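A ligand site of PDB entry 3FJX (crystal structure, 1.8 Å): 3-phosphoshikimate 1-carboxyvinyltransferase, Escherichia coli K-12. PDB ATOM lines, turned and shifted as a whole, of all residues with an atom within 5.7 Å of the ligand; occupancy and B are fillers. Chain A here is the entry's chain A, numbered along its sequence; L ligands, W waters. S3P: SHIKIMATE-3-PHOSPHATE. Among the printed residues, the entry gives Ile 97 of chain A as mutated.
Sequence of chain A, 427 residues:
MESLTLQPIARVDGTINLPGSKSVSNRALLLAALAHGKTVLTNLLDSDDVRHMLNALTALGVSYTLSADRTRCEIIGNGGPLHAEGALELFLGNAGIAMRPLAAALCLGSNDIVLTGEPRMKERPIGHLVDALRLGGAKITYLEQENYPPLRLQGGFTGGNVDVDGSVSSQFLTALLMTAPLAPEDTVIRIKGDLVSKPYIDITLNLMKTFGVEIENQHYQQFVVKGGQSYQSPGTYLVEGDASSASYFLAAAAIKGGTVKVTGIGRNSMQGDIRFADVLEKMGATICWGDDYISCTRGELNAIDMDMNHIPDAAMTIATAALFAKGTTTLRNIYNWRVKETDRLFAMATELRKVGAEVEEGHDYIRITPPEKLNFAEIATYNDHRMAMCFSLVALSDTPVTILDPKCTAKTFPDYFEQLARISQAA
The side-chain hydroxyl of Ser 197 sits at hydrogen-bond distance from an oxygen (O7) of the ligand (2.6 Å). NH1 of Arg 27 is in salt-bridge range of O4 of the ligand, at 2.7 Å. The backbone NH of Ser 170 lies within hydrogen-bond range of an oxygen (O6) of the ligand. An oxygen (O6) of the ligand is in hydrogen-bond range of the side-chain hydroxyl (OG) of Ser 170 (2.7 Å). The side-chain hydroxyl (OG) of Ser 23 lies within hydrogen-bond range of an oxygen (O5) of the ligand (2.7 Å). The side-chain hydroxyl (OG) of Ser 169 is in hydrogen-bond range of an oxygen (O8) of the ligand, 2.7 Å away. The side-chain carboxylate (OD1) of Asp 313 is in hydrogen-bond range of an oxygen (O3) of the ligand (2.7 Å). O7 of the ligand is in salt-bridge range of NZ of Lys 340. An oxygen (O7) of the ligand lies within hydrogen-bond range of the side-chain amide nitrogen of Asn 336 (2.9 Å). NE2 of Gln 171 lies within hydrogen-bond range of O1 of the ligand (3.0 Å). NZ of Lys 22 sits at hydrogen-bond distance from O3 of the ligand, at 3.0 Å.
Water W4 lies within hydrogen-bond range of O8 of the ligand (2.6 Å) and O of Val 168 (3.0 Å). Water W1 lies within hydrogen-bond range of an oxygen (O4) of the ligand (2.7 Å), the side-chain hydroxyl (OG1) of Thr 174 (2.8 Å), the side-chain hydroxyl (OG) of Ser 170 (2.8 Å), the guanidinium group (NH1) of Arg 27 (3.4 Å) and the backbone NH (N) of Gln 171 (3.4 Å). Water W3 lies within hydrogen-bond range of NE2 of Gln 171 (2.8 Å), O8 of the ligand (2.9 Å) and NH2 of Arg 100 (3.2 Å). Water W2 bridges the side-chain carboxylate of Glu 341 (2.9 Å) and an oxygen (O3) of the ligand (3.2 Å).
The backbone carbonyl oxygen of Ser 23 lies within hydrogen-bond range of the guanidinium group of Arg 27 (3.0 Å). The side-chain hydroxyl (OG1) of Thr 204 lies within hydrogen-bond range of the guanidinium group (NE) of Arg 27, at 2.8 Å. OD2 of Asp 313 is in salt-bridge range of NZ of Lys 340 (3.9 Å). The side-chain carboxylate (OD2) of Asp 313 is in salt-bridge range of the guanidinium group (NH2) of Arg 344 (3.5 Å). OD1 of Asp 313 is in salt-bridge range of NH1 of Arg 386, at 3.8 Å. The side-chain amino group (NZ) of Lys 340 lies within hydrogen-bond range of the side-chain amide oxygen (OD1) of Asn 336 (3.1 Å). The backbone carbonyl oxygen (O) of Val 168 sits at hydrogen-bond distance from the side-chain amide nitrogen (ND2) of Asn 336 (3.1 Å). The side-chain hydroxyl of Thr 204 sits at hydrogen-bond distance from the backbone carbonyl oxygen of Tyr 200 (3.2 Å).
Ile 97 touches the ligand (CD1 to O4, 3.6 Å). O of Val 168 touches O8 of the ligand, 3.99 Å away. CD2 of Tyr 200 touches C7 of the ligand (3.2 Å). Hydrophobic or aromatic side chains within 4 Å of the ligand: Ile 97 and Tyr 200. 13 residues have an atom within 4 Å of the ligand: Lys 22, Ser 23, Arg 27, Ile 97, Val 168, Ser 169, Ser 170, Gln 171, Ser 197, Tyr 200, Asp 313, Asn 336 and Lys 340. The nearest printed residue that does not touch the ligand is Pro 312 (4.2 Å).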
ATOM      1  N   LYS A  22      -5.806  15.520 -19.133  1.00  0.00           N
ATOM      2  CA  LYS A  22      -5.128  14.251 -18.871  1.00  0.00           C
ATOM      3  C   LYS A  22      -5.245  13.896 -17.386  1.00  0.00           C
ATOM      4  O   LYS A  22      -5.483  12.746 -17.029  1.00  0.00           O
ATOM      5  CB  LYS A  22      -3.653  14.345 -19.278  1.00  0.00           C
ATOM      6  CG  LYS A  22      -2.835  13.049 -19.017  1.00  0.00           C
ATOM      7  CD  LYS A  22      -1.848  13.229 -17.845  1.00  0.00           C
ATOM      8  CE  LYS A  22      -0.656  14.094 -18.273  1.00  0.00           C
ATOM      9  NZ  LYS A  22       0.165  14.616 -17.136  1.00  0.00           N
ATOM     10  N   SER A  23      -5.085  14.891 -16.538  1.00  0.00           N
ATOM     11  CA  SER A  23      -5.148  14.661 -15.087  1.00  0.00           C
ATOM     12  C   SER A  23      -6.509  14.137 -14.650  1.00  0.00           C
ATOM     13  O   SER A  23      -6.589  13.189 -13.871  1.00  0.00           O
ATOM     14  CB  SER A  23      -4.841  15.967 -14.343  1.00  0.00           C
ATOM     15  OG  SER A  23      -3.511  16.375 -14.605  1.00  0.00           O
ATOM     16  N   ARG A  27      -7.685   9.958 -13.662  1.00  0.00           N
ATOM     17  CA  ARG A  27      -8.282   9.789 -12.334  1.00  0.00           C
ATOM     18  C   ARG A  27      -9.709   9.233 -12.493  1.00  0.00           C
ATOM     19  O   ARG A  27     -10.116   8.320 -11.780  1.00  0.00           O
ATOM     20  CB  ARG A  27      -8.364  11.124 -11.601  1.00  0.00           C
ATOM     21  CG  ARG A  27      -7.065  11.604 -10.949  1.00  0.00           C
ATOM     22  CD  ARG A  27      -7.284  13.027 -10.442  1.00  0.00           C
ATOM     23  NE  ARG A  27      -6.160  13.586  -9.704  1.00  0.00           N
ATOM     24  CZ  ARG A  27      -5.015  13.993 -10.241  1.00  0.00           C
ATOM     25  NH1 ARG A  27      -4.074  14.498  -9.466  1.00  0.00           N
ATOM     26  NH2 ARG A  27      -4.802  13.905 -11.558  1.00  0.00           N
ATOM     27  N   ILE A  97       0.579   9.801 -14.055  1.00  0.00           N
ATOM     28  CA  ILE A  97      -0.737   9.750 -13.450  1.00  0.00           C
ATOM     29  C   ILE A  97      -1.416   8.386 -13.657  1.00  0.00           C
ATOM     30  O   ILE A  97      -2.562   8.193 -13.252  1.00  0.00           O
ATOM     31  CB  ILE A  97      -1.605  10.971 -13.899  1.00  0.00           C
ATOM     32  CG1 ILE A  97      -2.780  11.164 -12.925  1.00  0.00           C
ATOM     33  CG2 ILE A  97      -2.097  10.782 -15.317  1.00  0.00           C
ATOM     34  CD1 ILE A  97      -2.350  11.388 -11.460  1.00  0.00           C
ATOM     35  N   ARG A 100       1.611   6.131 -10.767  1.00  0.00           N
ATOM     36  CA  ARG A 100       1.502   6.390  -9.337  1.00  0.00           C
ATOM     37  C   ARG A 100       0.164   5.919  -8.758  1.00  0.00           C
ATOM     38  O   ARG A 100       0.146   5.145  -7.813  1.00  0.00           O
ATOM     39  CB  ARG A 100       1.796   7.878  -9.031  1.00  0.00           C
ATOM     40  CG  ARG A 100       3.314   8.221  -8.922  1.00  0.00           C
ATOM     41  CD  ARG A 100       4.079   8.062 -10.255  1.00  0.00           C
ATOM     42  NE  ARG A 100       5.480   8.518 -10.172  1.00  0.00           N
ATOM     43  CZ  ARG A 100       5.880   9.770 -10.369  1.00  0.00           C
ATOM     44  NH1 ARG A 100       7.159  10.073 -10.265  1.00  0.00           N
ATOM     45  NH2 ARG A 100       5.003  10.714 -10.678  1.00  0.00           N
ATOM     46  N   VAL A 168       8.588  16.056  -3.257  1.00  0.00           N
ATOM     47  CA  VAL A 168       9.025  15.798  -4.637  1.00  0.00           C
ATOM     48  C   VAL A 168       7.878  15.672  -5.633  1.00  0.00           C
ATOM     49  O   VAL A 168       7.954  16.178  -6.748  1.00  0.00           O
ATOM     50  CB  VAL A 168       9.901  14.534  -4.709  1.00  0.00           C
ATOM     51  CG1 VAL A 168      10.241  14.207  -6.151  1.00  0.00           C
ATOM     52  CG2 VAL A 168      11.191  14.778  -3.926  1.00  0.00           C
ATOM     53  N   SER A 169       6.809  14.999  -5.233  1.00  0.00           N
ATOM     54  CA  SER A 169       5.645  14.852  -6.110  1.00  0.00           C
ATOM     55  C   SER A 169       4.349  14.773  -5.325  1.00  0.00           C
ATOM     56  O   SER A 169       4.266  14.104  -4.300  1.00  0.00           O
ATOM     57  CB  SER A 169       5.786  13.583  -6.981  1.00  0.00           C
ATOM     58  OG  SER A 169       4.651  13.426  -7.829  1.00  0.00           O
ATOM     59  N   SER A 170       3.329  15.473  -5.815  1.00  0.00           N
ATOM     60  CA  SER A 170       2.030  15.412  -5.160  1.00  0.00           C
ATOM     61  C   SER A 170       1.345  14.122  -5.612  1.00  0.00           C
ATOM     62  O   SER A 170       0.367  13.694  -5.012  1.00  0.00           O
ATOM     63  CB  SER A 170       1.160  16.605  -5.574  1.00  0.00           C
ATOM     64  OG  SER A 170       0.817  16.517  -6.954  1.00  0.00           O
ATOM     65  N   GLN A 171       1.871  13.496  -6.662  1.00  0.00           N
ATOM     66  CA  GLN A 171       1.240  12.283  -7.158  1.00  0.00           C
ATOM     67  C   GLN A 171       1.236  11.154  -6.169  1.00  0.00           C
ATOM     68  O   GLN A 171       0.351  10.296  -6.203  1.00  0.00           O
ATOM     69  CB  GLN A 171       1.920  11.842  -8.441  1.00  0.00           C
ATOM     70  CG  GLN A 171       1.580  12.754  -9.590  1.00  0.00           C
ATOM     71  CD  GLN A 171       2.230  12.282 -10.871  1.00  0.00           C
ATOM     72  OE1 GLN A 171       2.248  11.091 -11.155  1.00  0.00           O
ATOM     73  NE2 GLN A 171       2.770  13.210 -11.638  1.00  0.00           N
ATOM     74  N   THR A 174      -1.689  11.830  -3.944  1.00  0.00           N
ATOM     75  CA  THR A 174      -2.898  11.604  -4.732  1.00  0.00           C
ATOM     76  C   THR A 174      -3.196  10.100  -4.787  1.00  0.00           C
ATOM     77  O   THR A 174      -4.332   9.666  -4.590  1.00  0.00           O
ATOM     78  CB  THR A 174      -2.703  12.155  -6.170  1.00  0.00           C
ATOM     79  OG1 THR A 174      -3.083  13.540  -6.184  1.00  0.00           O
ATOM     80  CG2 THR A 174      -3.512  11.374  -7.197  1.00  0.00           C
ATOM     81  N   VAL A 196       4.470  19.879  -2.583  1.00  0.00           N
ATOM     82  CA  VAL A 196       4.576  20.613  -3.846  1.00  0.00           C
ATOM     83  C   VAL A 196       3.372  20.296  -4.735  1.00  0.00           C
ATOM     84  O   VAL A 196       2.630  19.344  -4.485  1.00  0.00           O
ATOM     85  CB  VAL A 196       5.878  20.243  -4.599  1.00  0.00           C
ATOM     86  CG1 VAL A 196       7.109  20.742  -3.816  1.00  0.00           C
ATOM     87  CG2 VAL A 196       5.939  18.732  -4.809  1.00  0.00           C
ATOM     88  N   SER A 197       3.186  21.110  -5.775  1.00  0.00           N
ATOM     89  CA  SER A 197       2.075  20.910  -6.713  1.00  0.00           C
ATOM     90  C   SER A 197       0.731  20.713  -5.997  1.00  0.00           C
ATOM     91  O   SER A 197      -0.103  19.906  -6.394  1.00  0.00           O
ATOM     92  CB  SER A 197       2.357  19.686  -7.597  1.00  0.00           C
ATOM     93  OG  SER A 197       3.496  19.913  -8.404  1.00  0.00           O
ATOM     94  N   TYR A 200      -2.935  19.970  -7.502  1.00  0.00           N
ATOM     95  CA  TYR A 200      -3.304  18.672  -8.044  1.00  0.00           C
ATOM     96  C   TYR A 200      -3.971  17.835  -6.972  1.00  0.00           C
ATOM     97  O   TYR A 200      -4.761  16.936  -7.280  1.00  0.00           O
ATOM     98  CB  TYR A 200      -2.085  17.935  -8.619  1.00  0.00           C
ATOM     99  CG  TYR A 200      -1.646  18.535  -9.935  1.00  0.00           C
ATOM    100  CD1 TYR A 200      -0.604  19.462 -10.002  1.00  0.00           C
ATOM    101  CD2 TYR A 200      -2.314  18.205 -11.098  1.00  0.00           C
ATOM    102  CE1 TYR A 200      -0.231  20.045 -11.214  1.00  0.00           C
ATOM    103  CE2 TYR A 200      -1.950  18.771 -12.325  1.00  0.00           C
ATOM    104  CZ  TYR A 200      -0.909  19.693 -12.379  1.00  0.00           C
ATOM    105  OH  TYR A 200      -0.556  20.223 -13.612  1.00  0.00           O
ATOM    106  N   ILE A 203      -7.537  18.524  -7.239  1.00  0.00           N
ATOM    107  CA  ILE A 203      -8.159  17.835  -8.365  1.00  0.00           C
ATOM    108  C   ILE A 203      -8.558  16.436  -7.867  1.00  0.00           C
ATOM    109  O   ILE A 203      -9.669  15.974  -8.109  1.00  0.00           O
ATOM    110  CB  ILE A 203      -7.201  17.668  -9.583  1.00  0.00           C
ATOM    111  CG1 ILE A 203      -6.848  19.043 -10.161  1.00  0.00           C
ATOM    112  CG2 ILE A 203      -7.857  16.785 -10.654  1.00  0.00           C
ATOM    113  CD1 ILE A 203      -5.890  18.978 -11.350  1.00  0.00           C
ATOM    114  N   THR A 204      -7.640  15.780  -7.171  1.00  0.00           N
ATOM    115  CA  THR A 204      -7.898  14.443  -6.672  1.00  0.00           C
ATOM    116  C   THR A 204      -9.093  14.399  -5.733  1.00  0.00           C
ATOM    117  O   THR A 204      -9.972  13.558  -5.873  1.00  0.00           O
ATOM    118  CB  THR A 204      -6.649  13.901  -5.967  1.00  0.00           C
ATOM    119  OG1 THR A 204      -5.584  13.852  -6.926  1.00  0.00           O
ATOM    120  CG2 THR A 204      -6.889  12.495  -5.425  1.00  0.00           C
ATOM    121  N   PRO A 312       3.505  23.923 -12.170  1.00  0.00           N
ATOM    122  CA  PRO A 312       4.738  23.397 -12.787  1.00  0.00           C
ATOM    123  C   PRO A 312       4.700  23.060 -14.278  1.00  0.00           C
ATOM    124  O   PRO A 312       5.673  23.326 -14.990  1.00  0.00           O
ATOM    125  CB  PRO A 312       5.071  22.198 -11.902  1.00  0.00           C
ATOM    126  CG  PRO A 312       3.709  21.718 -11.441  1.00  0.00           C
ATOM    127  CD  PRO A 312       3.018  23.036 -11.098  1.00  0.00           C
ATOM    128  N   ASP A 313       3.601  22.498 -14.759  1.00  0.00           N
ATOM    129  CA  ASP A 313       3.518  22.150 -16.181  1.00  0.00           C
ATOM    130  C   ASP A 313       3.326  23.394 -17.057  1.00  0.00           C
ATOM    131  O   ASP A 313       4.149  23.665 -17.935  1.00  0.00           O
ATOM    132  CB  ASP A 313       2.375  21.162 -16.444  1.00  0.00           C
ATOM    133  CG  ASP A 313       2.666  19.763 -15.921  1.00  0.00           C
ATOM    134  OD1 ASP A 313       1.773  18.897 -15.996  1.00  0.00           O
ATOM    135  OD2 ASP A 313       3.789  19.528 -15.443  1.00  0.00           O
ATOM    136  N   ASN A 336      11.060  20.015  -9.143  1.00  0.00           N
ATOM    137  CA  ASN A 336      10.613  18.759  -9.719  1.00  0.00           C
ATOM    138  C   ASN A 336      10.468  18.678 -11.236  1.00  0.00           C
ATOM    139  O   ASN A 336      10.080  17.636 -11.776  1.00  0.00           O
ATOM    140  CB  ASN A 336       9.386  18.190  -8.990  1.00  0.00           C
ATOM    141  CG  ASN A 336       8.088  18.895  -9.321  1.00  0.00           C
ATOM    142  OD1 ASN A 336       8.004  19.714 -10.225  1.00  0.00           O
ATOM    143  ND2 ASN A 336       7.041  18.543  -8.561  1.00  0.00           N
ATOM    144  N   LYS A 340      10.565  14.753 -14.152  1.00  0.00           N
ATOM    145  CA  LYS A 340       9.375  14.505 -14.938  1.00  0.00           C
ATOM    146  C   LYS A 340       9.667  13.830 -16.277  1.00  0.00           C
ATOM    147  O   LYS A 340      10.586  13.031 -16.342  1.00  0.00           O
ATOM    148  CB  LYS A 340       8.591  15.801 -15.076  1.00  0.00           C
ATOM    149  CG  LYS A 340       7.779  16.024 -13.798  1.00  0.00           C
ATOM    150  CD  LYS A 340       7.200  17.383 -13.666  1.00  0.00           C
ATOM    151  CE  LYS A 340       6.357  17.418 -12.391  1.00  0.00           C
ATOM    152  NZ  LYS A 340       5.783  18.757 -12.161  1.00  0.00           N
ATOM    153  N   GLU A 341       8.887  14.115 -17.334  1.00  0.00           N
ATOM    154  CA  GLU A 341       9.106  13.463 -18.631  1.00  0.00           C
ATOM    155  C   GLU A 341      10.572  13.427 -19.056  1.00  0.00           C
ATOM    156  O   GLU A 341      11.014  12.482 -19.730  1.00  0.00           O
ATOM    157  CB  GLU A 341       8.209  14.111 -19.698  1.00  0.00           C
ATOM    158  CG  GLU A 341       6.752  13.595 -19.679  1.00  0.00           C
ATOM    159  CD  GLU A 341       5.847  14.277 -18.653  1.00  0.00           C
ATOM    160  OE1 GLU A 341       6.312  14.808 -17.594  1.00  0.00           O
ATOM    161  OE2 GLU A 341       4.629  14.272 -18.892  1.00  0.00           O
ATOM    162  N   ARG A 344      13.444  18.676 -17.139  1.00  0.00           N
ATOM    163  CA  ARG A 344      12.990  19.875 -17.821  1.00  0.00           C
ATOM    164  C   ARG A 344      13.816  21.134 -17.568  1.00  0.00           C
ATOM    165  O   ARG A 344      13.840  22.031 -18.415  1.00  0.00           O
ATOM    166  CB  ARG A 344      11.511  20.106 -17.499  1.00  0.00           C
ATOM    167  CG  ARG A 344      10.631  19.048 -18.180  1.00  0.00           C
ATOM    168  CD  ARG A 344       9.219  19.040 -17.655  1.00  0.00           C
ATOM    169  NE  ARG A 344       8.358  18.384 -18.632  1.00  0.00           N
ATOM    170  CZ  ARG A 344       7.074  18.112 -18.452  1.00  0.00           C
ATOM    171  NH1 ARG A 344       6.374  17.531 -19.422  1.00  0.00           N
ATOM    172  NH2 ARG A 344       6.489  18.399 -17.280  1.00  0.00           N
ATOM    173  N   ARG A 386       5.796  18.421 -23.821  1.00  0.00           N
ATOM    174  CA  ARG A 386       5.831  19.872 -23.545  1.00  0.00           C
ATOM    175  C   ARG A 386       7.010  20.616 -24.116  1.00  0.00           C
ATOM    176  O   ARG A 386       6.939  21.825 -24.318  1.00  0.00           O
ATOM    177  CB  ARG A 386       5.688  20.133 -22.040  1.00  0.00           C
ATOM    178  CG  ARG A 386       4.399  19.515 -21.467  1.00  0.00           C
ATOM    179  CD  ARG A 386       3.949  20.209 -20.146  1.00  0.00           C
ATOM    180  NE  ARG A 386       2.813  19.444 -19.641  1.00  0.00           N
ATOM    181  CZ  ARG A 386       1.601  19.457 -20.175  1.00  0.00           C
ATOM    182  NH1 ARG A 386       0.655  18.677 -19.641  1.00  0.00           N
ATOM    183  NH2 ARG A 386       1.292  20.274 -21.168  1.00  0.00           N
HETATM  184  C1  S3P L   1      -0.168  15.692 -12.155  1.00  0.00           C
HETATM  185  C2  S3P L   1       0.633  16.348 -11.181  1.00  0.00           C
HETATM  186  C3  S3P L   1       1.979  16.956 -11.536  1.00  0.00           C
HETATM  187  C4  S3P L   1       2.097  17.227 -13.059  1.00  0.00           C
HETATM  188  C5  S3P L   1       1.703  15.982 -13.869  1.00  0.00           C
HETATM  189  C6  S3P L   1       0.249  15.595 -13.523  1.00  0.00           C
HETATM  190  C7  S3P L   1      -1.500  15.118 -11.704  1.00  0.00           C
HETATM  191  O1  S3P L   1       3.124  16.115 -10.984  1.00  0.00           O
HETATM  192  O2  S3P L   1       3.438  17.667 -13.347  1.00  0.00           O
HETATM  193  O3  S3P L   1       1.813  16.267 -15.244  1.00  0.00           O
HETATM  194  O4  S3P L   1      -1.640  14.833 -10.497  1.00  0.00           O
HETATM  195  O5  S3P L   1      -2.396  15.043 -12.523  1.00  0.00           O
HETATM  196  P1  S3P L   1       3.970  16.500  -9.595  1.00  0.00           P
HETATM  197  O6  S3P L   1       3.072  16.399  -8.425  1.00  0.00           O
HETATM  198  O7  S3P L   1       4.460  17.907  -9.760  1.00  0.00           O
HETATM  199  O8  S3P L   1       5.088  15.555  -9.460  1.00  0.00           O
HETATM  200  O   HOH W   1      -1.130  14.660  -7.838  1.00  0.00           O
HETATM  201  O   HOH W   2       4.844  15.388 -15.116  1.00  0.00           O
HETATM  202  O   HOH W   3       5.509  13.670 -11.663  1.00  0.00           O
HETATM  203  O   HOH W   4       7.631  15.145  -9.498  1.00  0.00           O
